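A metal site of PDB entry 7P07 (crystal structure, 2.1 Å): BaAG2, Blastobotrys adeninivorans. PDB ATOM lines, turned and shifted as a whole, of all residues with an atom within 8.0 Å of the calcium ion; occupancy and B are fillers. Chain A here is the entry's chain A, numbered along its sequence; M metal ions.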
ATOM      1  N   PRO A  27      32.888  24.807  -7.093  1.00  0.00           N
ATOM      2  CA  PRO A  27      32.551  24.895  -5.672  1.00  0.00           C
ATOM      3  C   PRO A  27      31.098  25.168  -5.336  1.00  0.00           C
ATOM      4  O   PRO A  27      30.566  24.495  -4.531  1.00  0.00           O
ATOM      5  CB  PRO A  27      33.406  26.026  -5.121  1.00  0.00           C
ATOM      6  CG  PRO A  27      34.464  26.286  -6.150  1.00  0.00           C
ATOM      7  CD  PRO A  27      34.043  25.623  -7.424  1.00  0.00           C
ATOM      8  N   SER A  28      30.475  26.109  -6.025  1.00  0.00           N
ATOM      9  CA  SER A  28      29.083  26.517  -5.762  1.00  0.00           C
ATOM     10  C   SER A  28      28.094  25.414  -6.090  1.00  0.00           C
ATOM     11  O   SER A  28      27.068  25.403  -5.466  1.00  0.00           O
ATOM     12  CB  SER A  28      28.756  27.768  -6.505  1.00  0.00           C
ATOM     13  OG  SER A  28      28.228  27.473  -7.784  1.00  0.00           O
ATOM     14  N   LYS A  31      28.655  20.270  -3.825  1.00  0.00           N
ATOM     15  CA  LYS A  31      27.966  19.685  -2.645  1.00  0.00           C
ATOM     16  C   LYS A  31      27.826  20.722  -1.515  1.00  0.00           C
ATOM     17  O   LYS A  31      28.846  21.297  -1.143  1.00  0.00           O
ATOM     18  CB  LYS A  31      28.742  18.480  -2.128  1.00  0.00           C
ATOM     19  CG  LYS A  31      28.096  17.774  -0.942  1.00  0.00           C
ATOM     20  CD  LYS A  31      26.695  17.348  -1.224  1.00  0.00           C
ATOM     21  CE  LYS A  31      26.193  16.286  -0.280  1.00  0.00           C
ATOM     22  NZ  LYS A  31      25.252  16.845   0.707  1.00  0.00           N
ATOM     23  N   ASP A  32      26.622  20.934  -0.981  1.00  0.00           N
ATOM     24  CA  ASP A  32      26.305  21.848   0.134  1.00  0.00           C
ATOM     25  C   ASP A  32      26.247  20.990   1.400  1.00  0.00           C
ATOM     26  O   ASP A  32      25.502  20.034   1.409  1.00  0.00           O
ATOM     27  CB  ASP A  32      24.979  22.544  -0.156  1.00  0.00           C
ATOM     28  CG  ASP A  32      24.404  23.409   0.944  1.00  0.00           C
ATOM     29  OD1 ASP A  32      25.156  23.863   1.779  1.00  0.00           O
ATOM     30  OD2 ASP A  32      23.216  23.637   0.922  1.00  0.00           O
ATOM     31  N   SER A  33      26.985  21.331   2.441  1.00  0.00           N
ATOM     32  CA  SER A  33      27.051  20.560   3.704  1.00  0.00           C
ATOM     33  C   SER A  33      26.256  21.219   4.832  1.00  0.00           C
ATOM     34  O   SER A  33      26.223  20.618   5.893  1.00  0.00           O
ATOM     35  CB  SER A  33      28.469  20.394   4.114  1.00  0.00           C
ATOM     36  OG  SER A  33      29.016  21.621   4.538  1.00  0.00           O
ATOM     37  N   ASN A  34      25.588  22.366   4.618  1.00  0.00           N
ATOM     38  CA  ASN A  34      24.862  23.064   5.713  1.00  0.00           C
ATOM     39  C   ASN A  34      23.565  23.731   5.268  1.00  0.00           C
ATOM     40  O   ASN A  34      23.242  24.759   5.813  1.00  0.00           O
ATOM     41  CB  ASN A  34      25.740  24.126   6.355  1.00  0.00           C
ATOM     42  CG  ASN A  34      26.447  24.966   5.325  1.00  0.00           C
ATOM     43  OD1 ASN A  34      25.816  25.483   4.421  1.00  0.00           O
ATOM     44  ND2 ASN A  34      27.748  25.098   5.462  1.00  0.00           N
ATOM     45  N   GLY A  35      22.860  23.173   4.284  1.00  0.00           N
ATOM     46  CA  GLY A  35      21.524  23.589   3.808  1.00  0.00           C
ATOM     47  C   GLY A  35      21.304  25.050   3.484  1.00  0.00           C
ATOM     48  O   GLY A  35      20.148  25.440   3.487  1.00  0.00           O
ATOM     49  N   ASP A  36      22.324  25.842   3.159  1.00  0.00           N
ATOM     50  CA  ASP A  36      22.094  27.251   2.742  1.00  0.00           C
ATOM     51  C   ASP A  36      21.920  27.339   1.217  1.00  0.00           C
ATOM     52  O   ASP A  36      21.827  28.446   0.725  1.00  0.00           O
ATOM     53  CB  ASP A  36      23.214  28.168   3.224  1.00  0.00           C
ATOM     54  CG  ASP A  36      24.516  27.903   2.527  1.00  0.00           C
ATOM     55  OD1 ASP A  36      24.530  26.972   1.767  1.00  0.00           O
ATOM     56  OD2 ASP A  36      25.469  28.627   2.771  1.00  0.00           O
ATOM     57  N   GLY A  37      22.009  26.219   0.484  1.00  0.00           N
ATOM     58  CA  GLY A  37      21.770  26.127  -0.974  1.00  0.00           C
ATOM     59  C   GLY A  37      23.020  26.346  -1.792  1.00  0.00           C
ATOM     60  O   GLY A  37      22.944  26.216  -2.993  1.00  0.00           O
ATOM     61  N   ILE A  38      24.144  26.638  -1.164  1.00  0.00           N
ATOM     62  CA  ILE A  38      25.420  26.933  -1.853  1.00  0.00           C
ATOM     63  C   ILE A  38      26.369  25.782  -1.611  1.00  0.00           C
ATOM     64  O   ILE A  38      26.471  25.367  -0.495  1.00  0.00           O
ATOM     65  CB  ILE A  38      26.041  28.208  -1.266  1.00  0.00           C
ATOM     66  CG1 ILE A  38      25.009  29.331  -1.229  1.00  0.00           C
ATOM     67  CG2 ILE A  38      27.294  28.592  -2.013  1.00  0.00           C
ATOM     68  CD1 ILE A  38      25.059  30.187  -2.425  1.00  0.00           C
ATOM     69  N   GLY A  39      27.166  25.387  -2.583  1.00  0.00           N
ATOM     70  CA  GLY A  39      28.129  24.310  -2.382  1.00  0.00           C
ATOM     71  C   GLY A  39      29.286  24.805  -1.555  1.00  0.00           C
ATOM     72  O   GLY A  39      29.550  25.998  -1.595  1.00  0.00           O
ATOM     73  N   ASP A  40      30.016  23.933  -0.883  1.00  0.00           N
ATOM     74  CA  ASP A  40      31.116  24.430  -0.019  1.00  0.00           C
ATOM     75  C   ASP A  40      32.248  23.423   0.104  1.00  0.00           C
ATOM     76  O   ASP A  40      32.054  22.277  -0.272  1.00  0.00           O
ATOM     77  CB  ASP A  40      30.507  24.834   1.317  1.00  0.00           C
ATOM     78  CG  ASP A  40      29.721  23.684   1.897  1.00  0.00           C
ATOM     79  OD1 ASP A  40      30.281  22.655   2.102  1.00  0.00           O
ATOM     80  OD2 ASP A  40      28.556  23.822   2.109  1.00  0.00           O
ATOM     81  N   ILE A  41      33.384  23.876   0.624  1.00  0.00           N
ATOM     82  CA  ILE A  41      34.618  23.074   0.761  1.00  0.00           C
ATOM     83  C   ILE A  41      34.390  21.852   1.642  1.00  0.00           C
ATOM     84  O   ILE A  41      34.863  20.804   1.271  1.00  0.00           O
ATOM     85  CB  ILE A  41      35.786  23.957   1.201  1.00  0.00           C
ATOM     86  CG1 ILE A  41      36.125  24.987   0.123  1.00  0.00           C
ATOM     87  CG2 ILE A  41      36.962  23.101   1.563  1.00  0.00           C
ATOM     88  CD1 ILE A  41      37.124  25.994   0.547  1.00  0.00           C
ATOM     89  N   PRO A  42      33.647  21.884   2.774  1.00  0.00           N
ATOM     90  CA  PRO A  42      33.391  20.667   3.524  1.00  0.00           C
ATOM     91  C   PRO A  42      32.620  19.649   2.669  1.00  0.00           C
ATOM     92  O   PRO A  42      32.817  18.492   2.842  1.00  0.00           O
ATOM     93  CB  PRO A  42      32.566  21.120   4.725  1.00  0.00           C
ATOM     94  CG  PRO A  42      32.982  22.541   4.896  1.00  0.00           C
ATOM     95  CD  PRO A  42      33.135  23.043   3.476  1.00  0.00           C
ATOM     96  N   GLY A  43      31.681  20.108   1.850  1.00  0.00           N
ATOM     97  CA  GLY A  43      30.970  19.234   0.909  1.00  0.00           C
ATOM     98  C   GLY A  43      31.957  18.564  -0.019  1.00  0.00           C
ATOM     99  O   GLY A  43      31.861  17.382  -0.207  1.00  0.00           O
ATOM    100  N   GLU A  84      33.540  33.359   1.812  1.00  0.00           N
ATOM    101  CA  GLU A  84      32.993  32.956   3.132  1.00  0.00           C
ATOM    102  C   GLU A  84      31.987  31.816   2.988  1.00  0.00           C
ATOM    103  O   GLU A  84      32.107  30.879   3.770  1.00  0.00           O
ATOM    104  CB  GLU A  84      32.536  34.222   3.872  1.00  0.00           C
ATOM    105  CG  GLU A  84      33.677  35.155   4.180  1.00  0.00           C
ATOM    106  CD  GLU A  84      34.125  35.963   2.971  1.00  0.00           C
ATOM    107  OE1 GLU A  84      35.301  36.359   2.916  1.00  0.00           O
ATOM    108  OE2 GLU A  84      33.296  36.157   2.077  1.00  0.00           O
ATOM    109  N   PRO A  85      30.982  31.799   2.091  1.00  0.00           N
ATOM    110  CA  PRO A  85      30.102  30.643   1.946  1.00  0.00           C
ATOM    111  C   PRO A  85      30.778  29.298   1.646  1.00  0.00           C
ATOM    112  O   PRO A  85      30.232  28.305   1.994  1.00  0.00           O
ATOM    113  CB  PRO A  85      29.223  30.993   0.752  1.00  0.00           C
ATOM    114  CG  PRO A  85      29.129  32.469   0.787  1.00  0.00           C
ATOM    115  CD  PRO A  85      30.461  32.923   1.329  1.00  0.00           C
ATOM    116  N   TYR A  86      31.913  29.310   0.962  1.00  0.00           N
ATOM    117  CA  TYR A  86      32.686  28.084   0.638  1.00  0.00           C
ATOM    118  C   TYR A  86      33.292  27.572   1.936  1.00  0.00           C
ATOM    119  O   TYR A  86      33.371  26.360   2.109  1.00  0.00           O
ATOM    120  CB  TYR A  86      33.683  28.352  -0.485  1.00  0.00           C
ATOM    121  CG  TYR A  86      33.056  28.625  -1.823  1.00  0.00           C
ATOM    122  CD1 TYR A  86      31.750  28.269  -2.094  1.00  0.00           C
ATOM    123  CD2 TYR A  86      33.762  29.256  -2.825  1.00  0.00           C
ATOM    124  CE1 TYR A  86      31.159  28.533  -3.305  1.00  0.00           C
ATOM    125  CE2 TYR A  86      33.192  29.541  -4.046  1.00  0.00           C
ATOM    126  CZ  TYR A  86      31.882  29.174  -4.282  1.00  0.00           C
ATOM    127  OH  TYR A  86      31.296  29.438  -5.484  1.00  0.00           O
ATOM    128  N   GLY A  87      33.669  28.466   2.850  1.00  0.00           N
ATOM    129  CA  GLY A  87      34.229  28.103   4.155  1.00  0.00           C
ATOM    130  C   GLY A  87      35.378  28.985   4.548  1.00  0.00           C
ATOM    131  O   GLY A  87      35.653  29.922   3.852  1.00  0.00           O
ATOM    132  N   PHE A 457      21.762  17.320  -3.200  1.00  0.00           N
ATOM    133  CA  PHE A 457      22.855  18.304  -3.245  1.00  0.00           C
ATOM    134  C   PHE A 457      22.738  19.222  -2.045  1.00  0.00           C
ATOM    135  O   PHE A 457      23.740  19.730  -1.564  1.00  0.00           O
ATOM    136  CB  PHE A 457      22.786  19.142  -4.519  1.00  0.00           C
ATOM    137  CG  PHE A 457      23.441  20.489  -4.410  1.00  0.00           C
ATOM    138  CD1 PHE A 457      24.799  20.623  -4.430  1.00  0.00           C
ATOM    139  CD2 PHE A 457      22.667  21.630  -4.346  1.00  0.00           C
ATOM    140  CE1 PHE A 457      25.387  21.867  -4.365  1.00  0.00           C
ATOM    141  CE2 PHE A 457      23.242  22.879  -4.287  1.00  0.00           C
ATOM    142  CZ  PHE A 457      24.604  22.990  -4.297  1.00  0.00           C
ATOM    143  N   THR A 458      21.521  19.437  -1.571  1.00  0.00           N
ATOM    144  CA  THR A 458      21.322  20.337  -0.421  1.00  0.00           C
ATOM    145  C   THR A 458      20.006  20.062   0.319  1.00  0.00           C
ATOM    146  O   THR A 458      19.079  19.614  -0.328  1.00  0.00           O
ATOM    147  CB  THR A 458      21.240  21.785  -0.894  1.00  0.00           C
ATOM    148  OG1 THR A 458      21.034  22.516   0.297  1.00  0.00           O
ATOM    149  CG2 THR A 458      20.143  22.053  -1.879  1.00  0.00           C
HETATM  150 CA    CA M   1      26.880  25.818   2.072  1.00  0.00          CA
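Along chain A the residues within 4 Å of the calcium ion span positions 32 to 40.
OD1 of Asn 34 binds the calcium ion, at 2.6 Å.
The side-chain carboxylate (OD2) of Asp 40 binds the calcium ion, 2.6 Å away.
OD1 of Asp 32 binds the calcium ion.
The calcium ion is bound by the side-chain carboxylate (OD1) of Asp 36.
The calcium ion is bound by O of Ile 38, 2.6 Å away.
OG of Ser 33 lies within hydrogen-bond range of OD1 of Asp 40.
The backbone NH (N) of Asp 40 sits at hydrogen-bond distance from the backbone carbonyl oxygen (O) of Lys 31, 2.9 Å away.
The backbone NH (N) of Gly 43 is in hydrogen-bond range of the side-chain carboxylate (OD1) of Asp 40 (2.9 Å).
The side-chain carboxylate of Asp 32 lies within hydrogen-bond range of the backbone NH of Gly 37 (2.9 Å).
N of Gly 35 sits close to OD2 of Asp 32, at 3.4 Å.
OD2 of Asp 32 lies within hydrogen-bond range of OG1 of Thr 458 (2.5 Å).
O of Phe 457 sits at hydrogen-bond distance from N of Asp 32 (3.2 Å).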
